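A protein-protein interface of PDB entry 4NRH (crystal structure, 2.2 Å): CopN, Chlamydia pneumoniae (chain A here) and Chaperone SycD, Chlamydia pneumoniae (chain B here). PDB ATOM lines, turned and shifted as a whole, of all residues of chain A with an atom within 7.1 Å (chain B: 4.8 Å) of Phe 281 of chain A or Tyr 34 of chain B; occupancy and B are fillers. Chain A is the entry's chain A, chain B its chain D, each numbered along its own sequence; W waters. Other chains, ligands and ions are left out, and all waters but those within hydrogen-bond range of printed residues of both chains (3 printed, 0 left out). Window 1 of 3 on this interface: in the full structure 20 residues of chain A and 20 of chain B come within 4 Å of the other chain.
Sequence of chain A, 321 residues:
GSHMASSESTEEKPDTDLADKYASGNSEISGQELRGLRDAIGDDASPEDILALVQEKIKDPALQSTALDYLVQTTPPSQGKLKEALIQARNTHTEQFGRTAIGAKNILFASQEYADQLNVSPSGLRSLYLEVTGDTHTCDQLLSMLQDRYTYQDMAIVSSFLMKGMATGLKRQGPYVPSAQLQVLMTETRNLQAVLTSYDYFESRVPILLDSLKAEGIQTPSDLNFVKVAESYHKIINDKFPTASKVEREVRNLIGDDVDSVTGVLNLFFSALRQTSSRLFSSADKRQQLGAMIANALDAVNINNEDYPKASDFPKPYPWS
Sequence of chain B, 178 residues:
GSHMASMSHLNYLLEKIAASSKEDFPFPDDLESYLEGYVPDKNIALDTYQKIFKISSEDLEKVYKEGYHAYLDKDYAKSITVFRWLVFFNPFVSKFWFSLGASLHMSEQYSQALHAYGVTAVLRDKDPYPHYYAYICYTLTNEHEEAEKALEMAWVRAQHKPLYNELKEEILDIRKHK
O of Tyr 34 of chain B lies within hydrogen-bond range of N of Ala 284 of chain A (2.9 Å). The guanidinium group of Arg 287 of chain A is in hydrogen-bond range of the side-chain hydroxyl of Tyr 49 of chain B (3.0 Å).
Printed residues of chain A that touch a printed residue of chain B: Ser 278, Phe 281, Ser 282, Ser 283, Ala 284 and Arg 287. Hydrophobic or aromatic side chains of chain A within 4 Å of the printed part of chain B: Ala 284. Of the 10 printed residues of chain B, 4 touch a printed residue of chain A. Hydrophobic or aromatic side chains of chain B that line the printed part of chain A: Pro 28, Tyr 34, Tyr 49 and Phe 88. Among the printed residues, 8 pairs touch across the chains.
Among the printed residues, merely in contact across the chains: Ser 278 of chain A with Tyr 49 of chain B, Phe 281 of chain A with Tyr 34 of chain B, Ser 283 of chain A with Tyr 34 of chain B, Ser 278 of chain A with Pro 28 of chain B, Ser 282 of chain A with Tyr 34 of chain B and Ser 278 of chain A with Phe 88 of chain B.
O of Leu 273 of chain A sits at hydrogen-bond distance from NH2 of Arg 287 of chain A (3.0 Å). The side-chain hydroxyl of Ser 283 of chain A is in hydrogen-bond range of the backbone NH of Lys 286 of chain A, at 3.2 Å.
Of the printed residues of chain B, Ser 278 of chain A touches Pro 28 (3.5 Å), Tyr 49 (3.3 Å) and Phe 88 (3.6 Å). Printed residues of chain B within 4 Å of Ser 282 of chain A: Tyr 34 (3.6 Å). Gln 288 of chain A touches none of the printed residues of chain B. Of the printed residues of chain A, Pro 28 of chain B touches Ser 278 (3.5 Å). Leu 35 of chain B touches none of the printed residues of chain A. The nearest residue of chain A that does not touch Tyr 34 of chain B is Arg 287 of chain A (4.4 Å). The nearest printed residue of chain A that does not touch Phe 88 of chain B is Arg 279 of chain A (6.5 Å).
Water W1 lies within hydrogen-bond range of the side-chain hydroxyl (OH) of Tyr 34 of chain B (2.6 Å), the side-chain hydroxyl (OH) of Tyr 49 of chain B (2.7 Å) and the backbone carbonyl oxygen (O) of Ser 278 of chain A (2.8 Å). Water W2 lies within hydrogen-bond range of the backbone carbonyl oxygen of Leu 273 of chain A, the side-chain hydroxyl of Tyr 49 of chain B and the backbone carbonyl oxygen of Thr 276 of chain A. Water W3 lies within hydrogen-bond range of O of Tyr 34 of chain B (2.7 Å), N of Asp 285 of chain A (2.9 Å), O of Glu 36 of chain B (3.2 Å) and N of Ala 284 of chain A (3.2 Å).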
ATOM      1  N   ALA A 194     -10.367 -17.290 -38.951  1.00  0.00           N
ATOM      2  CA  ALA A 194     -10.561 -17.393 -37.510  1.00  0.00           C
ATOM      3  C   ALA A 194      -9.692 -16.371 -36.785  1.00  0.00           C
ATOM      4  O   ALA A 194     -10.150 -15.680 -35.874  1.00  0.00           O
ATOM      5  CB  ALA A 194     -10.247 -18.801 -37.026  1.00  0.00           C
ATOM      6  N   TYR A 233      -3.000 -11.942 -27.352  1.00  0.00           N
ATOM      7  CA  TYR A 233      -4.130 -12.860 -27.239  1.00  0.00           C
ATOM      8  C   TYR A 233      -3.813 -14.205 -27.885  1.00  0.00           C
ATOM      9  O   TYR A 233      -4.071 -15.260 -27.307  1.00  0.00           O
ATOM     10  CB  TYR A 233      -5.374 -12.233 -27.875  1.00  0.00           C
ATOM     11  CG  TYR A 233      -6.630 -13.071 -27.800  1.00  0.00           C
ATOM     12  CD1 TYR A 233      -7.170 -13.448 -26.576  1.00  0.00           C
ATOM     13  CD2 TYR A 233      -7.296 -13.459 -28.955  1.00  0.00           C
ATOM     14  CE1 TYR A 233      -8.327 -14.206 -26.507  1.00  0.00           C
ATOM     15  CE2 TYR A 233      -8.452 -14.211 -28.899  1.00  0.00           C
ATOM     16  CZ  TYR A 233      -8.964 -14.584 -27.673  1.00  0.00           C
ATOM     17  OH  TYR A 233     -10.115 -15.338 -27.617  1.00  0.00           O
ATOM     18  N   ILE A 237      -3.279 -17.868 -26.296  1.00  0.00           N
ATOM     19  CA  ILE A 237      -4.065 -18.995 -26.794  1.00  0.00           C
ATOM     20  C   ILE A 237      -3.163 -20.138 -27.255  1.00  0.00           C
ATOM     21  O   ILE A 237      -3.443 -21.310 -26.997  1.00  0.00           O
ATOM     22  CB  ILE A 237      -4.984 -18.570 -27.961  1.00  0.00           C
ATOM     23  CG1 ILE A 237      -6.163 -17.748 -27.441  1.00  0.00           C
ATOM     24  CG2 ILE A 237      -5.506 -19.782 -28.717  1.00  0.00           C
ATOM     25  CD1 ILE A 237      -7.171 -17.404 -28.514  1.00  0.00           C
ATOM     26  N   PHE A 269      -9.702  -9.977 -22.719  1.00  0.00           N
ATOM     27  CA  PHE A 269      -9.282 -11.312 -23.133  1.00  0.00           C
ATOM     28  C   PHE A 269     -10.344 -12.360 -22.819  1.00  0.00           C
ATOM     29  O   PHE A 269     -10.622 -13.236 -23.639  1.00  0.00           O
ATOM     30  CB  PHE A 269      -7.960 -11.696 -22.462  1.00  0.00           C
ATOM     31  CG  PHE A 269      -6.748 -11.087 -23.111  1.00  0.00           C
ATOM     32  CD1 PHE A 269      -6.863 -10.363 -24.285  1.00  0.00           C
ATOM     33  CD2 PHE A 269      -5.493 -11.246 -22.548  1.00  0.00           C
ATOM     34  CE1 PHE A 269      -5.749  -9.805 -24.884  1.00  0.00           C
ATOM     35  CE2 PHE A 269      -4.375 -10.691 -23.141  1.00  0.00           C
ATOM     36  CZ  PHE A 269      -4.503  -9.969 -24.312  1.00  0.00           C
ATOM     37  N   ALA A 272     -13.234 -12.111 -25.052  1.00  0.00           N
ATOM     38  CA  ALA A 272     -12.858 -12.556 -26.391  1.00  0.00           C
ATOM     39  C   ALA A 272     -13.106 -14.050 -26.589  1.00  0.00           C
ATOM     40  O   ALA A 272     -13.268 -14.516 -27.717  1.00  0.00           O
ATOM     41  CB  ALA A 272     -11.398 -12.225 -26.667  1.00  0.00           C
ATOM     42  N   LEU A 273     -13.131 -14.798 -25.489  1.00  0.00           N
ATOM     43  CA  LEU A 273     -13.304 -16.247 -25.554  1.00  0.00           C
ATOM     44  C   LEU A 273     -14.689 -16.646 -26.056  1.00  0.00           C
ATOM     45  O   LEU A 273     -14.879 -17.758 -26.551  1.00  0.00           O
ATOM     46  CB  LEU A 273     -13.054 -16.871 -24.180  1.00  0.00           C
ATOM     47  CG  LEU A 273     -11.658 -16.664 -23.590  1.00  0.00           C
ATOM     48  CD1 LEU A 273     -11.606 -17.168 -22.159  1.00  0.00           C
ATOM     49  CD2 LEU A 273     -10.607 -17.354 -24.441  1.00  0.00           C
ATOM     50  N   ARG A 274     -15.653 -15.739 -25.927  1.00  0.00           N
ATOM     51  CA  ARG A 274     -17.001 -15.992 -26.426  1.00  0.00           C
ATOM     52  C   ARG A 274     -17.352 -15.130 -27.634  1.00  0.00           C
ATOM     53  O   ARG A 274     -18.449 -15.242 -28.180  1.00  0.00           O
ATOM     54  CB  ARG A 274     -18.031 -15.764 -25.319  1.00  0.00           C
ATOM     55  CG  ARG A 274     -18.232 -14.305 -24.949  1.00  0.00           C
ATOM     56  CD  ARG A 274     -19.481 -14.119 -24.105  1.00  0.00           C
ATOM     57  NE  ARG A 274     -19.494 -12.830 -23.422  1.00  0.00           N
ATOM     58  CZ  ARG A 274     -20.007 -11.718 -23.939  1.00  0.00           C
ATOM     59  NH1 ARG A 274     -20.546 -11.736 -25.151  1.00  0.00           N
ATOM     60  NH2 ARG A 274     -19.978 -10.587 -23.247  1.00  0.00           N
ATOM     61  N   THR A 276     -14.804 -14.470 -30.197  1.00  0.00           N
ATOM     62  CA  THR A 276     -13.932 -14.843 -31.302  1.00  0.00           C
ATOM     63  C   THR A 276     -14.231 -16.266 -31.767  1.00  0.00           C
ATOM     64  O   THR A 276     -14.913 -17.023 -31.076  1.00  0.00           O
ATOM     65  CB  THR A 276     -12.445 -14.723 -30.919  1.00  0.00           C
ATOM     66  OG1 THR A 276     -12.174 -15.540 -29.774  1.00  0.00           O
ATOM     67  CG2 THR A 276     -12.092 -13.278 -30.597  1.00  0.00           C
ATOM     68  N   SER A 277     -13.721 -16.612 -32.943  1.00  0.00           N
ATOM     69  CA  SER A 277     -14.029 -17.883 -33.589  1.00  0.00           C
ATOM     70  C   SER A 277     -13.637 -19.099 -32.755  1.00  0.00           C
ATOM     71  O   SER A 277     -12.570 -19.128 -32.143  1.00  0.00           O
ATOM     72  CB  SER A 277     -13.340 -17.959 -34.951  1.00  0.00           C
ATOM     73  OG  SER A 277     -13.520 -19.237 -35.539  1.00  0.00           O
ATOM     74  N   SER A 278     -14.518 -20.096 -32.737  1.00  0.00           N
ATOM     75  CA  SER A 278     -14.268 -21.345 -32.028  1.00  0.00           C
ATOM     76  C   SER A 278     -13.089 -22.096 -32.639  1.00  0.00           C
ATOM     77  O   SER A 278     -12.433 -22.896 -31.971  1.00  0.00           O
ATOM     78  CB  SER A 278     -15.516 -22.228 -32.047  1.00  0.00           C
ATOM     79  OG  SER A 278     -15.758 -22.753 -33.341  1.00  0.00           O
ATOM     80  N   ARG A 279     -12.830 -21.831 -33.915  1.00  0.00           N
ATOM     81  CA  ARG A 279     -11.750 -22.481 -34.650  1.00  0.00           C
ATOM     82  C   ARG A 279     -10.372 -22.094 -34.108  1.00  0.00           C
ATOM     83  O   ARG A 279      -9.387 -22.795 -34.336  1.00  0.00           O
ATOM     84  CB  ARG A 279     -11.852 -22.134 -36.137  1.00  0.00           C
ATOM     85  CG  ARG A 279     -11.025 -23.019 -37.050  1.00  0.00           C
ATOM     86  CD  ARG A 279     -11.237 -22.643 -38.505  1.00  0.00           C
ATOM     87  NE  ARG A 279     -10.385 -23.420 -39.400  1.00  0.00           N
ATOM     88  CZ  ARG A 279     -10.717 -24.604 -39.901  1.00  0.00           C
ATOM     89  NH1 ARG A 279     -11.884 -25.153 -39.592  1.00  0.00           N
ATOM     90  NH2 ARG A 279      -9.881 -25.240 -40.710  1.00  0.00           N
ATOM     91  N   LEU A 280     -10.312 -20.976 -33.390  1.00  0.00           N
ATOM     92  CA  LEU A 280      -9.074 -20.510 -32.768  1.00  0.00           C
ATOM     93  C   LEU A 280      -8.502 -21.507 -31.763  1.00  0.00           C
ATOM     94  O   LEU A 280      -7.301 -21.510 -31.496  1.00  0.00           O
ATOM     95  CB  LEU A 280      -9.306 -19.173 -32.065  1.00  0.00           C
ATOM     96  CG  LEU A 280      -9.466 -17.934 -32.940  1.00  0.00           C
ATOM     97  CD1 LEU A 280      -9.647 -16.717 -32.058  1.00  0.00           C
ATOM     98  CD2 LEU A 280      -8.262 -17.769 -33.849  1.00  0.00           C
ATOM     99  N   PHE A 281      -9.367 -22.351 -31.209  1.00  0.00           N
ATOM    100  CA  PHE A 281      -8.958 -23.278 -30.161  1.00  0.00           C
ATOM    101  C   PHE A 281      -8.923 -24.717 -30.670  1.00  0.00           C
ATOM    102  O   PHE A 281      -9.921 -25.235 -31.171  1.00  0.00           O
ATOM    103  CB  PHE A 281      -9.897 -23.159 -28.957  1.00  0.00           C
ATOM    104  CG  PHE A 281     -10.031 -21.754 -28.433  1.00  0.00           C
ATOM    105  CD1 PHE A 281     -10.978 -20.890 -28.960  1.00  0.00           C
ATOM    106  CD2 PHE A 281      -9.200 -21.294 -27.424  1.00  0.00           C
ATOM    107  CE1 PHE A 281     -11.100 -19.597 -28.486  1.00  0.00           C
ATOM    108  CE2 PHE A 281      -9.318 -20.002 -26.945  1.00  0.00           C
ATOM    109  CZ  PHE A 281     -10.268 -19.153 -27.478  1.00  0.00           C
ATOM    110  N   SER A 282      -7.763 -25.353 -30.538  1.00  0.00           N
ATOM    111  CA  SER A 282      -7.566 -26.714 -31.025  1.00  0.00           C
ATOM    112  C   SER A 282      -8.172 -27.763 -30.097  1.00  0.00           C
ATOM    113  O   SER A 282      -8.298 -28.929 -30.470  1.00  0.00           O
ATOM    114  CB  SER A 282      -6.073 -26.994 -31.214  1.00  0.00           C
ATOM    115  OG  SER A 282      -5.359 -26.752 -30.014  1.00  0.00           O
ATOM    116  N   SER A 283      -8.540 -27.351 -28.889  1.00  0.00           N
ATOM    117  CA  SER A 283      -9.204 -28.254 -27.955  1.00  0.00           C
ATOM    118  C   SER A 283     -10.116 -27.511 -26.987  1.00  0.00           C
ATOM    119  O   SER A 283      -9.815 -26.394 -26.567  1.00  0.00           O
ATOM    120  CB  SER A 283      -8.167 -29.064 -27.173  1.00  0.00           C
ATOM    121  OG  SER A 283      -7.685 -28.334 -26.061  1.00  0.00           O
ATOM    122  N   ALA A 284     -11.237 -28.139 -26.643  1.00  0.00           N
ATOM    123  CA  ALA A 284     -12.176 -27.580 -25.677  1.00  0.00           C
ATOM    124  C   ALA A 284     -11.542 -27.439 -24.298  1.00  0.00           C
ATOM    125  O   ALA A 284     -11.859 -26.515 -23.549  1.00  0.00           O
ATOM    126  CB  ALA A 284     -13.427 -28.442 -25.595  1.00  0.00           C
ATOM    127  N   ASP A 285     -10.649 -28.368 -23.971  1.00  0.00           N
ATOM    128  CA  ASP A 285      -9.986 -28.387 -22.672  1.00  0.00           C
ATOM    129  C   ASP A 285      -9.162 -27.126 -22.405  1.00  0.00           C
ATOM    130  O   ASP A 285      -9.233 -26.553 -21.318  1.00  0.00           O
ATOM    131  CB  ASP A 285      -9.092 -29.625 -22.566  1.00  0.00           C
ATOM    132  CG  ASP A 285      -8.338 -29.693 -21.252  1.00  0.00           C
ATOM    133  OD1 ASP A 285      -8.910 -29.291 -20.216  1.00  0.00           O
ATOM    134  OD2 ASP A 285      -7.178 -30.155 -21.253  1.00  0.00           O
ATOM    135  N   LYS A 286      -8.387 -26.697 -23.396  1.00  0.00           N
ATOM    136  CA  LYS A 286      -7.512 -25.538 -23.238  1.00  0.00           C
ATOM    137  C   LYS A 286      -8.282 -24.224 -23.210  1.00  0.00           C
ATOM    138  O   LYS A 286      -7.941 -23.323 -22.443  1.00  0.00           O
ATOM    139  CB  LYS A 286      -6.465 -25.499 -24.348  1.00  0.00           C
ATOM    140  CG  LYS A 286      -5.330 -26.480 -24.144  1.00  0.00           C
ATOM    141  CD  LYS A 286      -4.421 -26.513 -25.352  1.00  0.00           C
ATOM    142  CE  LYS A 286      -3.811 -27.884 -25.504  1.00  0.00           C
ATOM    143  NZ  LYS A 286      -3.085 -28.038 -26.791  1.00  0.00           N
ATOM    144  N   ARG A 287      -9.306 -24.114 -24.052  1.00  0.00           N
ATOM    145  CA  ARG A 287     -10.190 -22.953 -24.025  1.00  0.00           C
ATOM    146  C   ARG A 287     -10.779 -22.777 -22.630  1.00  0.00           C
ATOM    147  O   ARG A 287     -10.753 -21.682 -22.067  1.00  0.00           O
ATOM    148  CB  ARG A 287     -11.312 -23.094 -25.054  1.00  0.00           C
ATOM    149  CG  ARG A 287     -12.395 -22.038 -24.911  1.00  0.00           C
ATOM    150  CD  ARG A 287     -13.400 -22.095 -26.046  1.00  0.00           C
ATOM    151  NE  ARG A 287     -14.356 -20.995 -25.965  1.00  0.00           N
ATOM    152  CZ  ARG A 287     -15.512 -21.060 -25.315  1.00  0.00           C
ATOM    153  NH1 ARG A 287     -15.855 -22.174 -24.683  1.00  0.00           N
ATOM    154  NH2 ARG A 287     -16.325 -20.011 -25.292  1.00  0.00           N
ATOM    155  N   GLN A 288     -11.315 -23.864 -22.086  1.00  0.00           N
ATOM    156  CA  GLN A 288     -11.862 -23.863 -20.734  1.00  0.00           C
ATOM    157  C   GLN A 288     -10.793 -23.513 -19.701  1.00  0.00           C
ATOM    158  O   GLN A 288     -11.022 -22.694 -18.810  1.00  0.00           O
ATOM    159  CB  GLN A 288     -12.478 -25.224 -20.408  1.00  0.00           C
ATOM    160  CG  GLN A 288     -12.914 -25.378 -18.963  1.00  0.00           C
ATOM    161  CD  GLN A 288     -13.707 -26.648 -18.727  1.00  0.00           C
ATOM    162  OE1 GLN A 288     -14.937 -26.625 -18.673  1.00  0.00           O
ATOM    163  NE2 GLN A 288     -13.005 -27.766 -18.589  1.00  0.00           N
ATOM    164  N   LEU A 290      -8.024 -21.893 -20.203  1.00  0.00           N
ATOM    165  CA  LEU A 290      -7.571 -20.520 -20.394  1.00  0.00           C
ATOM    166  C   LEU A 290      -8.536 -19.544 -19.731  1.00  0.00           C
ATOM    167  O   LEU A 290      -8.116 -18.552 -19.136  1.00  0.00           O
ATOM    168  CB  LEU A 290      -7.425 -20.194 -21.881  1.00  0.00           C
ATOM    169  CG  LEU A 290      -6.912 -18.784 -22.166  1.00  0.00           C
ATOM    170  CD1 LEU A 290      -5.640 -18.540 -21.375  1.00  0.00           C
ATOM    171  CD2 LEU A 290      -6.670 -18.577 -23.654  1.00  0.00           C
ATOM    172  N   PRO B  28     -14.143 -25.982 -35.492  1.00  0.00           N
ATOM    173  CA  PRO B  28     -12.981 -26.869 -35.621  1.00  0.00           C
ATOM    174  C   PRO B  28     -13.206 -27.918 -36.708  1.00  0.00           C
ATOM    175  O   PRO B  28     -14.337 -28.363 -36.903  1.00  0.00           O
ATOM    176  CB  PRO B  28     -12.873 -27.517 -34.237  1.00  0.00           C
ATOM    177  CG  PRO B  28     -13.577 -26.573 -33.317  1.00  0.00           C
ATOM    178  CD  PRO B  28     -14.692 -25.986 -34.125  1.00  0.00           C
ATOM    179  N   ASP B  30     -11.863 -30.951 -36.720  1.00  0.00           N
ATOM    180  CA  ASP B  30     -11.810 -32.295 -36.159  1.00  0.00           C
ATOM    181  C   ASP B  30     -12.345 -32.289 -34.730  1.00  0.00           C
ATOM    182  O   ASP B  30     -11.593 -32.081 -33.779  1.00  0.00           O
ATOM    183  CB  ASP B  30     -10.375 -32.832 -36.197  1.00  0.00           C
ATOM    184  CG  ASP B  30     -10.285 -34.315 -35.866  1.00  0.00           C
ATOM    185  OD1 ASP B  30     -11.260 -34.885 -35.335  1.00  0.00           O
ATOM    186  OD2 ASP B  30      -9.224 -34.914 -36.139  1.00  0.00           O
ATOM    187  N   LEU B  31     -13.647 -32.514 -34.589  1.00  0.00           N
ATOM    188  CA  LEU B  31     -14.289 -32.491 -33.277  1.00  0.00           C
ATOM    189  C   LEU B  31     -13.812 -33.633 -32.380  1.00  0.00           C
ATOM    190  O   LEU B  31     -13.860 -33.522 -31.157  1.00  0.00           O
ATOM    191  CB  LEU B  31     -15.810 -32.545 -33.424  1.00  0.00           C
ATOM    192  CG  LEU B  31     -16.477 -31.260 -33.921  1.00  0.00           C
ATOM    193  CD1 LEU B  31     -17.990 -31.380 -33.846  1.00  0.00           C
ATOM    194  CD2 LEU B  31     -15.992 -30.058 -33.123  1.00  0.00           C
ATOM    195  N   GLU B  32     -13.358 -34.726 -32.985  1.00  0.00           N
ATOM    196  CA  GLU B  32     -12.808 -35.839 -32.218  1.00  0.00           C
ATOM    197  C   GLU B  32     -11.556 -35.406 -31.462  1.00  0.00           C
ATOM    198  O   GLU B  32     -11.410 -35.676 -30.271  1.00  0.00           O
ATOM    199  CB  GLU B  32     -12.485 -37.025 -33.126  1.00  0.00           C
ATOM    200  CG  GLU B  32     -11.944 -38.225 -32.371  1.00  0.00           C
ATOM    201  CD  GLU B  32     -11.467 -39.336 -33.284  1.00  0.00           C
ATOM    202  OE1 GLU B  32     -11.661 -39.229 -34.512  1.00  0.00           O
ATOM    203  OE2 GLU B  32     -10.891 -40.318 -32.769  1.00  0.00           O
ATOM    204  N   SER B  33     -10.655 -34.733 -32.169  1.00  0.00           N
ATOM    205  CA  SER B  33      -9.417 -34.241 -31.578  1.00  0.00           C
ATOM    206  C   SER B  33      -9.709 -33.098 -30.611  1.00  0.00           C
ATOM    207  O   SER B  33      -9.047 -32.948 -29.585  1.00  0.00           O
ATOM    208  CB  SER B  33      -8.447 -33.784 -32.667  1.00  0.00           C
ATOM    209  OG  SER B  33      -7.287 -33.199 -32.104  1.00  0.00           O
ATOM    210  N   TYR B  34     -10.701 -32.288 -30.965  1.00  0.00           N
ATOM    211  CA  TYR B  34     -11.092 -31.124 -30.178  1.00  0.00           C
ATOM    212  C   TYR B  34     -11.663 -31.517 -28.814  1.00  0.00           C
ATOM    213  O   TYR B  34     -11.511 -30.788 -27.835  1.00  0.00           O
ATOM    214  CB  TYR B  34     -12.104 -30.288 -30.969  1.00  0.00           C
ATOM    215  CG  TYR B  34     -12.662 -29.086 -30.238  1.00  0.00           C
ATOM    216  CD1 TYR B  34     -11.997 -27.867 -30.260  1.00  0.00           C
ATOM    217  CD2 TYR B  34     -13.872 -29.160 -29.559  1.00  0.00           C
ATOM    218  CE1 TYR B  34     -12.506 -26.762 -29.606  1.00  0.00           C
ATOM    219  CE2 TYR B  34     -14.391 -28.059 -28.904  1.00  0.00           C
ATOM    220  CZ  TYR B  34     -13.703 -26.863 -28.929  1.00  0.00           C
ATOM    221  OH  TYR B  34     -14.213 -25.763 -28.277  1.00  0.00           O
ATOM    222  N   LEU B  35     -12.317 -32.674 -28.756  1.00  0.00           N
ATOM    223  CA  LEU B  35     -13.001 -33.115 -27.543  1.00  0.00           C
ATOM    224  C   LEU B  35     -12.172 -34.084 -26.698  1.00  0.00           C
ATOM    225  O   LEU B  35     -12.593 -34.475 -25.609  1.00  0.00           O
ATOM    226  CB  LEU B  35     -14.341 -33.763 -27.898  1.00  0.00           C
ATOM    227  CG  LEU B  35     -15.416 -32.832 -28.463  1.00  0.00           C
ATOM    228  CD1 LEU B  35     -16.617 -33.627 -28.949  1.00  0.00           C
ATOM    229  CD2 LEU B  35     -15.831 -31.798 -27.428  1.00  0.00           C
ATOM    230  N   GLU B  36     -11.012 -34.487 -27.207  1.00  0.00           N
ATOM    231  CA  GLU B  36     -10.161 -35.450 -26.507  1.00  0.00           C
ATOM    232  C   GLU B  36      -9.690 -34.930 -25.148  1.00  0.00           C
ATOM    233  O   GLU B  36      -9.148 -33.829 -25.046  1.00  0.00           O
ATOM    234  CB  GLU B  36      -8.952 -35.817 -27.375  1.00  0.00           C
ATOM    235  CG  GLU B  36      -8.340 -37.180 -27.066  1.00  0.00           C
ATOM    236  CD  GLU B  36      -7.540 -37.203 -25.776  1.00  0.00           C
ATOM    237  OE1 GLU B  36      -6.949 -36.161 -25.419  1.00  0.00           O
ATOM    238  OE2 GLU B  36      -7.501 -38.265 -25.119  1.00  0.00           O
ATOM    239  N   TYR B  49     -21.270 -22.674 -26.580  1.00  0.00           N
ATOM    240  CA  TYR B  49     -21.438 -22.238 -27.962  1.00  0.00           C
ATOM    241  C   TYR B  49     -22.908 -22.247 -28.374  1.00  0.00           C
ATOM    242  O   TYR B  49     -23.294 -21.552 -29.313  1.00  0.00           O
ATOM    243  CB  TYR B  49     -20.592 -23.095 -28.905  1.00  0.00           C
ATOM    244  CG  TYR B  49     -19.136 -22.683 -28.885  1.00  0.00           C
ATOM    245  CD1 TYR B  49     -18.752 -21.421 -29.316  1.00  0.00           C
ATOM    246  CD2 TYR B  49     -18.152 -23.543 -28.418  1.00  0.00           C
ATOM    247  CE1 TYR B  49     -17.429 -21.027 -29.293  1.00  0.00           C
ATOM    248  CE2 TYR B  49     -16.823 -23.159 -28.391  1.00  0.00           C
ATOM    249  CZ  TYR B  49     -16.468 -21.899 -28.830  1.00  0.00           C
ATOM    250  OH  TYR B  49     -15.150 -21.509 -28.809  1.00  0.00           O
ATOM    251  N   PHE B  88     -20.285 -30.310 -28.561  1.00  0.00           N
ATOM    252  CA  PHE B  88     -19.585 -29.073 -28.891  1.00  0.00           C
ATOM    253  C   PHE B  88     -20.422 -27.850 -28.527  1.00  0.00           C
ATOM    254  O   PHE B  88     -19.904 -26.865 -28.002  1.00  0.00           O
ATOM    255  CB  PHE B  88     -19.221 -29.048 -30.381  1.00  0.00           C
ATOM    256  CG  PHE B  88     -18.772 -27.701 -30.878  1.00  0.00           C
ATOM    257  CD1 PHE B  88     -17.453 -27.303 -30.739  1.00  0.00           C
ATOM    258  CD2 PHE B  88     -19.662 -26.843 -31.507  1.00  0.00           C
ATOM    259  CE1 PHE B  88     -17.034 -26.068 -31.199  1.00  0.00           C
ATOM    260  CE2 PHE B  88     -19.249 -25.608 -31.969  1.00  0.00           C
ATOM    261  CZ  PHE B  88     -17.933 -25.220 -31.816  1.00  0.00           C
HETATM  262  O   HOH W   1     -13.365 -23.521 -29.376  1.00  0.00           O
HETATM  263  O   HOH W   2     -14.559 -18.881 -28.976  1.00  0.00           O
HETATM  264  O   HOH W   3     -10.530 -30.984 -25.306  1.00  0.00           O
